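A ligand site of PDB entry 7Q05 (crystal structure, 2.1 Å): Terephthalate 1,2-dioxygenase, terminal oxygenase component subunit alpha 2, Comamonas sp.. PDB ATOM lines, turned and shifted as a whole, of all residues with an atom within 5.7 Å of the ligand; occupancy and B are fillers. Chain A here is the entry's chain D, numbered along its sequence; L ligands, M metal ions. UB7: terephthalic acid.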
ATOM      1  N   TYR A 203     -16.875  18.251 -22.702  1.00  0.00           N
ATOM      2  CA  TYR A 203     -18.342  18.446 -22.772  1.00  0.00           C
ATOM      3  C   TYR A 203     -18.636  19.822 -23.382  1.00  0.00           C
ATOM      4  O   TYR A 203     -19.519  19.900 -24.237  1.00  0.00           O
ATOM      5  CB  TYR A 203     -19.077  18.259 -21.445  1.00  0.00           C
ATOM      6  CG  TYR A 203     -20.565  18.428 -21.651  1.00  0.00           C
ATOM      7  CD1 TYR A 203     -21.371  17.425 -22.157  1.00  0.00           C
ATOM      8  CD2 TYR A 203     -21.159  19.652 -21.398  1.00  0.00           C
ATOM      9  CE1 TYR A 203     -22.736  17.604 -22.326  1.00  0.00           C
ATOM     10  CE2 TYR A 203     -22.500  19.875 -21.630  1.00  0.00           C
ATOM     11  CZ  TYR A 203     -23.299  18.844 -22.061  1.00  0.00           C
ATOM     12  OH  TYR A 203     -24.626  19.083 -22.258  1.00  0.00           O
ATOM     13  N   ASN A 206     -18.225  19.653 -26.918  1.00  0.00           N
ATOM     14  CA  ASN A 206     -19.318  18.818 -27.489  1.00  0.00           C
ATOM     15  C   ASN A 206     -20.542  19.710 -27.728  1.00  0.00           C
ATOM     16  O   ASN A 206     -21.165  19.574 -28.776  1.00  0.00           O
ATOM     17  CB  ASN A 206     -19.688  17.634 -26.601  1.00  0.00           C
ATOM     18  CG  ASN A 206     -20.696  16.727 -27.272  1.00  0.00           C
ATOM     19  OD1 ASN A 206     -20.369  16.085 -28.259  1.00  0.00           O
ATOM     20  ND2 ASN A 206     -21.937  16.753 -26.837  1.00  0.00           N
ATOM     21  N   VAL A 207     -20.853  20.606 -26.802  1.00  0.00           N
ATOM     22  CA  VAL A 207     -22.055  21.484 -26.916  1.00  0.00           C
ATOM     23  C   VAL A 207     -21.894  22.353 -28.175  1.00  0.00           C
ATOM     24  O   VAL A 207     -22.899  22.669 -28.821  1.00  0.00           O
ATOM     25  CB  VAL A 207     -22.231  22.379 -25.670  1.00  0.00           C
ATOM     26  CG1 VAL A 207     -23.425  23.279 -25.889  1.00  0.00           C
ATOM     27  CG2 VAL A 207     -22.444  21.607 -24.405  1.00  0.00           C
ATOM     28  N   LYS A 208     -20.655  22.776 -28.455  1.00  0.00           N
ATOM     29  CA  LYS A 208     -20.305  23.713 -29.566  1.00  0.00           C
ATOM     30  C   LYS A 208     -20.080  22.929 -30.859  1.00  0.00           C
ATOM     31  O   LYS A 208     -19.773  23.579 -31.907  1.00  0.00           O
ATOM     32  CB  LYS A 208     -19.083  24.542 -29.173  1.00  0.00           C
ATOM     33  CG  LYS A 208     -19.247  25.422 -27.951  1.00  0.00           C
ATOM     34  CD  LYS A 208     -17.955  25.969 -27.423  1.00  0.00           C
ATOM     35  CE  LYS A 208     -18.151  26.970 -26.295  1.00  0.00           C
ATOM     36  NZ  LYS A 208     -18.826  28.186 -26.804  1.00  0.00           N
ATOM     37  N   ASP A 209     -20.236  21.608 -30.831  1.00  0.00           N
ATOM     38  CA  ASP A 209     -19.763  20.753 -31.950  1.00  0.00           C
ATOM     39  C   ASP A 209     -20.924  20.553 -32.916  1.00  0.00           C
ATOM     40  O   ASP A 209     -21.531  19.480 -32.886  1.00  0.00           O
ATOM     41  CB  ASP A 209     -19.066  19.510 -31.416  1.00  0.00           C
ATOM     42  CG  ASP A 209     -18.428  18.594 -32.435  1.00  0.00           C
ATOM     43  OD1 ASP A 209     -18.592  18.818 -33.649  1.00  0.00           O
ATOM     44  OD2 ASP A 209     -17.812  17.646 -32.000  1.00  0.00           O
ATOM     45  N   SER A 210     -21.103  21.505 -33.847  1.00  0.00           N
ATOM     46  CA  SER A 210     -22.199  21.447 -34.853  1.00  0.00           C
ATOM     47  C   SER A 210     -21.974  20.262 -35.776  1.00  0.00           C
ATOM     48  O   SER A 210     -22.959  19.687 -36.254  1.00  0.00           O
ATOM     49  CB  SER A 210     -22.319  22.762 -35.608  1.00  0.00           C
ATOM     50  OG  SER A 210     -21.114  23.044 -36.344  1.00  0.00           O
ATOM     51  N   HIS A 212     -20.807  17.168 -35.057  1.00  0.00           N
ATOM     52  CA  HIS A 212     -21.277  15.905 -34.442  1.00  0.00           C
ATOM     53  C   HIS A 212     -22.800  15.803 -34.421  1.00  0.00           C
ATOM     54  O   HIS A 212     -23.295  14.637 -34.546  1.00  0.00           O
ATOM     55  CB  HIS A 212     -20.614  15.714 -33.080  1.00  0.00           C
ATOM     56  CG  HIS A 212     -21.545  15.872 -31.956  1.00  0.00           C
ATOM     57  ND1 HIS A 212     -21.791  17.114 -31.376  1.00  0.00           N
ATOM     58  CD2 HIS A 212     -22.293  14.954 -31.329  1.00  0.00           C
ATOM     59  CE1 HIS A 212     -22.668  16.949 -30.409  1.00  0.00           C
ATOM     60  NE2 HIS A 212     -22.980  15.602 -30.359  1.00  0.00           N
ATOM     61  N   ALA A 213     -23.574  16.889 -34.238  1.00  0.00           N
ATOM     62  CA  ALA A 213     -25.046  16.827 -33.927  1.00  0.00           C
ATOM     63  C   ALA A 213     -25.805  15.719 -34.682  1.00  0.00           C
ATOM     64  O   ALA A 213     -26.461  14.887 -34.023  1.00  0.00           O
ATOM     65  CB  ALA A 213     -25.702  18.139 -34.175  1.00  0.00           C
ATOM     66  N   HIS A 217     -25.908  11.456 -33.127  1.00  0.00           N
ATOM     67  CA  HIS A 217     -27.359  11.321 -32.810  1.00  0.00           C
ATOM     68  C   HIS A 217     -28.179  10.908 -34.042  1.00  0.00           C
ATOM     69  O   HIS A 217     -28.564  11.819 -34.854  1.00  0.00           O
ATOM     70  CB  HIS A 217     -27.903  12.617 -32.222  1.00  0.00           C
ATOM     71  CG  HIS A 217     -27.054  13.176 -31.139  1.00  0.00           C
ATOM     72  ND1 HIS A 217     -26.690  12.413 -30.043  1.00  0.00           N
ATOM     73  CD2 HIS A 217     -26.541  14.403 -30.948  1.00  0.00           C
ATOM     74  CE1 HIS A 217     -25.995  13.165 -29.214  1.00  0.00           C
ATOM     75  NE2 HIS A 217     -25.889  14.394 -29.743  1.00  0.00           N
ATOM     76  N   PHE A 220     -31.451  12.848 -34.448  1.00  0.00           N
ATOM     77  CA  PHE A 220     -31.299  14.169 -35.131  1.00  0.00           C
ATOM     78  C   PHE A 220     -31.359  14.039 -36.674  1.00  0.00           C
ATOM     79  O   PHE A 220     -31.858  14.987 -37.315  1.00  0.00           O
ATOM     80  CB  PHE A 220     -29.990  14.875 -34.729  1.00  0.00           C
ATOM     81  CG  PHE A 220     -30.063  15.934 -33.646  1.00  0.00           C
ATOM     82  CD1 PHE A 220     -31.234  16.624 -33.370  1.00  0.00           C
ATOM     83  CD2 PHE A 220     -28.929  16.264 -32.924  1.00  0.00           C
ATOM     84  CE1 PHE A 220     -31.266  17.586 -32.370  1.00  0.00           C
ATOM     85  CE2 PHE A 220     -28.956  17.239 -31.937  1.00  0.00           C
ATOM     86  CZ  PHE A 220     -30.130  17.898 -31.649  1.00  0.00           C
ATOM     87  N   HIS A 243     -21.302  30.527 -28.393  1.00  0.00           N
ATOM     88  CA  HIS A 243     -21.828  30.150 -29.733  1.00  0.00           C
ATOM     89  C   HIS A 243     -23.349  30.039 -29.678  1.00  0.00           C
ATOM     90  O   HIS A 243     -23.933  30.017 -28.568  1.00  0.00           O
ATOM     91  CB  HIS A 243     -21.130  28.904 -30.291  1.00  0.00           C
ATOM     92  CG  HIS A 243     -21.942  27.656 -30.216  1.00  0.00           C
ATOM     93  ND1 HIS A 243     -22.421  27.161 -29.017  1.00  0.00           N
ATOM     94  CD2 HIS A 243     -22.311  26.783 -31.181  1.00  0.00           C
ATOM     95  CE1 HIS A 243     -23.108  26.070 -29.250  1.00  0.00           C
ATOM     96  NE2 HIS A 243     -23.077  25.811 -30.570  1.00  0.00           N
ATOM     97  N   SER A 245     -25.868  27.446 -32.141  1.00  0.00           N
ATOM     98  CA  SER A 245     -26.126  26.554 -33.290  1.00  0.00           C
ATOM     99  C   SER A 245     -27.634  26.511 -33.452  1.00  0.00           C
ATOM    100  O   SER A 245     -28.346  26.373 -32.444  1.00  0.00           O
ATOM    101  CB  SER A 245     -25.486  25.218 -33.071  1.00  0.00           C
ATOM    102  OG  SER A 245     -25.733  24.391 -34.210  1.00  0.00           O
ATOM    103  N   TYR A 246     -28.136  26.729 -34.644  1.00  0.00           N
ATOM    104  CA  TYR A 246     -29.606  26.826 -34.872  1.00  0.00           C
ATOM    105  C   TYR A 246     -29.990  26.134 -36.171  1.00  0.00           C
ATOM    106  O   TYR A 246     -29.168  25.962 -37.070  1.00  0.00           O
ATOM    107  CB  TYR A 246     -30.074  28.276 -34.830  1.00  0.00           C
ATOM    108  CG  TYR A 246     -29.581  29.104 -35.985  1.00  0.00           C
ATOM    109  CD1 TYR A 246     -28.339  29.716 -35.960  1.00  0.00           C
ATOM    110  CD2 TYR A 246     -30.356  29.251 -37.110  1.00  0.00           C
ATOM    111  CE1 TYR A 246     -27.871  30.452 -37.041  1.00  0.00           C
ATOM    112  CE2 TYR A 246     -29.917  30.016 -38.186  1.00  0.00           C
ATOM    113  CZ  TYR A 246     -28.671  30.611 -38.148  1.00  0.00           C
ATOM    114  OH  TYR A 246     -28.241  31.373 -39.201  1.00  0.00           O
ATOM    115  N   LEU A 290     -34.573  24.277 -33.532  1.00  0.00           N
ATOM    116  CA  LEU A 290     -33.424  23.994 -32.628  1.00  0.00           C
ATOM    117  C   LEU A 290     -32.574  25.242 -32.429  1.00  0.00           C
ATOM    118  O   LEU A 290     -32.164  25.839 -33.435  1.00  0.00           O
ATOM    119  CB  LEU A 290     -32.605  22.846 -33.220  1.00  0.00           C
ATOM    120  CG  LEU A 290     -31.514  22.323 -32.284  1.00  0.00           C
ATOM    121  CD1 LEU A 290     -31.482  20.813 -32.248  1.00  0.00           C
ATOM    122  CD2 LEU A 290     -30.145  22.896 -32.646  1.00  0.00           C
ATOM    123  N   ILE A 292     -29.242  25.915 -29.729  1.00  0.00           N
ATOM    124  CA  ILE A 292     -28.299  25.637 -28.631  1.00  0.00           C
ATOM    125  C   ILE A 292     -27.404  26.855 -28.489  1.00  0.00           C
ATOM    126  O   ILE A 292     -26.770  27.261 -29.476  1.00  0.00           O
ATOM    127  CB  ILE A 292     -27.469  24.374 -28.912  1.00  0.00           C
ATOM    128  CG1 ILE A 292     -28.353  23.219 -29.350  1.00  0.00           C
ATOM    129  CG2 ILE A 292     -26.701  23.991 -27.646  1.00  0.00           C
ATOM    130  CD1 ILE A 292     -29.269  22.730 -28.239  1.00  0.00           C
ATOM    131  N   VAL A 300     -25.227  26.649 -20.766  1.00  0.00           N
ATOM    132  CA  VAL A 300     -25.965  26.243 -21.993  1.00  0.00           C
ATOM    133  C   VAL A 300     -27.443  26.637 -21.813  1.00  0.00           C
ATOM    134  O   VAL A 300     -28.005  26.390 -20.715  1.00  0.00           O
ATOM    135  CB  VAL A 300     -25.834  24.752 -22.279  1.00  0.00           C
ATOM    136  CG1 VAL A 300     -26.519  24.384 -23.580  1.00  0.00           C
ATOM    137  CG2 VAL A 300     -24.379  24.344 -22.337  1.00  0.00           C
ATOM    138  N   GLN A 302     -30.926  25.745 -24.013  1.00  0.00           N
ATOM    139  CA  GLN A 302     -31.366  24.887 -25.133  1.00  0.00           C
ATOM    140  C   GLN A 302     -32.843  25.116 -25.393  1.00  0.00           C
ATOM    141  O   GLN A 302     -33.659  25.212 -24.435  1.00  0.00           O
ATOM    142  CB  GLN A 302     -31.092  23.388 -24.944  1.00  0.00           C
ATOM    143  CG  GLN A 302     -31.903  22.791 -23.830  1.00  0.00           C
ATOM    144  CD  GLN A 302     -32.362  21.356 -24.021  1.00  0.00           C
ATOM    145  OE1 GLN A 302     -31.570  20.435 -23.788  1.00  0.00           O
ATOM    146  NE2 GLN A 302     -33.659  21.178 -24.286  1.00  0.00           N
ATOM    147  N   ILE A 304     -35.056  22.824 -28.031  1.00  0.00           N
ATOM    148  CA  ILE A 304     -35.262  21.721 -29.023  1.00  0.00           C
ATOM    149  C   ILE A 304     -36.754  21.511 -29.128  1.00  0.00           C
ATOM    150  O   ILE A 304     -37.344  21.020 -28.166  1.00  0.00           O
ATOM    151  CB  ILE A 304     -34.500  20.455 -28.591  1.00  0.00           C
ATOM    152  CG1 ILE A 304     -33.025  20.774 -28.355  1.00  0.00           C
ATOM    153  CG2 ILE A 304     -34.712  19.347 -29.604  1.00  0.00           C
ATOM    154  CD1 ILE A 304     -32.201  19.678 -27.689  1.00  0.00           C
ATOM    155  N   ARG A 311     -28.365  24.336 -18.786  1.00  0.00           N
ATOM    156  CA  ARG A 311     -27.321  23.441 -18.222  1.00  0.00           C
ATOM    157  C   ARG A 311     -26.216  24.269 -17.624  1.00  0.00           C
ATOM    158  O   ARG A 311     -25.829  25.289 -18.219  1.00  0.00           O
ATOM    159  CB  ARG A 311     -26.732  22.503 -19.266  1.00  0.00           C
ATOM    160  CG  ARG A 311     -27.773  22.006 -20.253  1.00  0.00           C
ATOM    161  CD  ARG A 311     -27.152  21.163 -21.322  1.00  0.00           C
ATOM    162  NE  ARG A 311     -28.069  21.017 -22.425  1.00  0.00           N
ATOM    163  CZ  ARG A 311     -27.733  20.691 -23.661  1.00  0.00           C
ATOM    164  NH1 ARG A 311     -28.700  20.543 -24.552  1.00  0.00           N
ATOM    165  NH2 ARG A 311     -26.461  20.451 -24.007  1.00  0.00           N
ATOM    166  N   ILE A 354     -31.561  12.047 -27.664  1.00  0.00           N
ATOM    167  CA  ILE A 354     -30.444  12.852 -28.231  1.00  0.00           C
ATOM    168  C   ILE A 354     -29.279  12.829 -27.253  1.00  0.00           C
ATOM    169  O   ILE A 354     -28.158  12.435 -27.644  1.00  0.00           O
ATOM    170  CB  ILE A 354     -30.861  14.314 -28.508  1.00  0.00           C
ATOM    171  CG1 ILE A 354     -31.919  14.404 -29.600  1.00  0.00           C
ATOM    172  CG2 ILE A 354     -29.642  15.182 -28.818  1.00  0.00           C
ATOM    173  CD1 ILE A 354     -31.671  13.392 -30.649  1.00  0.00           C
ATOM    174  N   SER A 355     -29.473  13.290 -26.036  1.00  0.00           N
ATOM    175  CA  SER A 355     -28.313  13.739 -25.230  1.00  0.00           C
ATOM    176  C   SER A 355     -27.627  12.608 -24.459  1.00  0.00           C
ATOM    177  O   SER A 355     -26.584  12.889 -23.816  1.00  0.00           O
ATOM    178  CB  SER A 355     -28.712  14.878 -24.342  1.00  0.00           C
ATOM    179  OG  SER A 355     -29.869  14.549 -23.663  1.00  0.00           O
ATOM    180  N   ASP A 358     -24.190  12.273 -25.551  1.00  0.00           N
ATOM    181  CA  ASP A 358     -23.349  13.418 -25.138  1.00  0.00           C
ATOM    182  C   ASP A 358     -22.749  13.093 -23.757  1.00  0.00           C
ATOM    183  O   ASP A 358     -21.657  13.530 -23.465  1.00  0.00           O
ATOM    184  CB  ASP A 358     -24.110  14.738 -25.124  1.00  0.00           C
ATOM    185  CG  ASP A 358     -24.755  15.133 -26.438  1.00  0.00           C
ATOM    186  OD1 ASP A 358     -24.075  14.909 -27.511  1.00  0.00           O
ATOM    187  OD2 ASP A 358     -25.931  15.695 -26.378  1.00  0.00           O
ATOM    188  N   ARG A 392     -23.266  24.007 -40.941  1.00  0.00           N
ATOM    189  CA  ARG A 392     -22.951  23.359 -39.646  1.00  0.00           C
ATOM    190  C   ARG A 392     -21.912  22.227 -39.783  1.00  0.00           C
ATOM    191  O   ARG A 392     -21.434  21.723 -38.709  1.00  0.00           O
ATOM    192  CB  ARG A 392     -24.275  22.972 -38.983  1.00  0.00           C
ATOM    193  CG  ARG A 392     -25.006  24.204 -38.451  1.00  0.00           C
ATOM    194  CD  ARG A 392     -26.358  24.013 -37.806  1.00  0.00           C
ATOM    195  NE  ARG A 392     -27.146  23.061 -38.590  1.00  0.00           N
ATOM    196  CZ  ARG A 392     -28.051  22.231 -38.103  1.00  0.00           C
ATOM    197  NH1 ARG A 392     -28.368  22.263 -36.819  1.00  0.00           N
ATOM    198  NH2 ARG A 392     -28.647  21.383 -38.935  1.00  0.00           N
HETATM  199  C01 UB7 L   1     -25.120  20.987 -30.480  1.00  0.00           C
HETATM  200  C02 UB7 L   1     -25.359  20.521 -29.198  1.00  0.00           C
HETATM  201  C03 UB7 L   1     -26.607  19.968 -28.847  1.00  0.00           C
HETATM  202  C04 UB7 L   1     -27.590  19.860 -29.833  1.00  0.00           C
HETATM  203  C05 UB7 L   1     -27.367  20.342 -31.120  1.00  0.00           C
HETATM  204  C06 UB7 L   1     -26.126  20.923 -31.460  1.00  0.00           C
HETATM  205  C07 UB7 L   1     -25.885  21.547 -32.803  1.00  0.00           C
HETATM  206  C10 UB7 L   1     -26.886  19.605 -27.417  1.00  0.00           C
HETATM  207  O08 UB7 L   1     -24.959  22.369 -32.957  1.00  0.00           O
HETATM  208  O09 UB7 L   1     -26.696  21.188 -33.761  1.00  0.00           O
HETATM  209  O11 UB7 L   1     -28.148  19.210 -27.161  1.00  0.00           O
HETATM  210  O12 UB7 L   1     -25.986  19.684 -26.517  1.00  0.00           O
HETATM  211 FE    FE M   1     -24.905  16.410 -28.996  1.00  0.00          FE
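The side-chain hydroxyl (OG) of Ser 245 sits at hydrogen-bond distance from an oxygen (O08) of the ligand (2.5 Å).
The guanidinium group (NH2) of Arg 311 is in salt-bridge range of an oxygen (O12) of the ligand (2.7 Å).
NH1 of Arg 392 lies within salt-bridge range of O09 of the ligand (3.6 Å).
The backbone NH (N) of Ser 245 lies within hydrogen-bond range of the backbone carbonyl oxygen (O) of Ile 292 (2.8 Å).
OH of Tyr 203 lies within hydrogen-bond range of NH2 of Arg 311, at 2.9 Å.
The guanidinium group (NH1) of Arg 311 is in hydrogen-bond range of the side-chain amide oxygen (OE1) of Gln 302 (3.0 Å).
O of Val 300 is in hydrogen-bond range of N of Arg 311 (2.8 Å).
The side-chain hydroxyl (OG) of Ser 210 sits at hydrogen-bond distance from the backbone carbonyl oxygen (O) of Arg 392 (2.7 Å).
The side-chain carboxylate of Asp 358 lies close to the side-chain amide nitrogen of Asn 206 (2.9 Å).
Val 207 touches the ligand.
CA of Ser 210 touches O08 of the ligand, at 3.5 Å.
CB of Ala 213 touches O09 of the ligand, 3.2 Å away.
Phe 220 touches the ligand.
Ile 292 touches the ligand.
Asp 358 touches the ligand (OD2 to O12, 3.99 Å).
Of the 23 residues printed, 9 come within 4 Å of the ligand.
Along chain A the residues within 4 Å of the ligand span positions 207 to 392.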
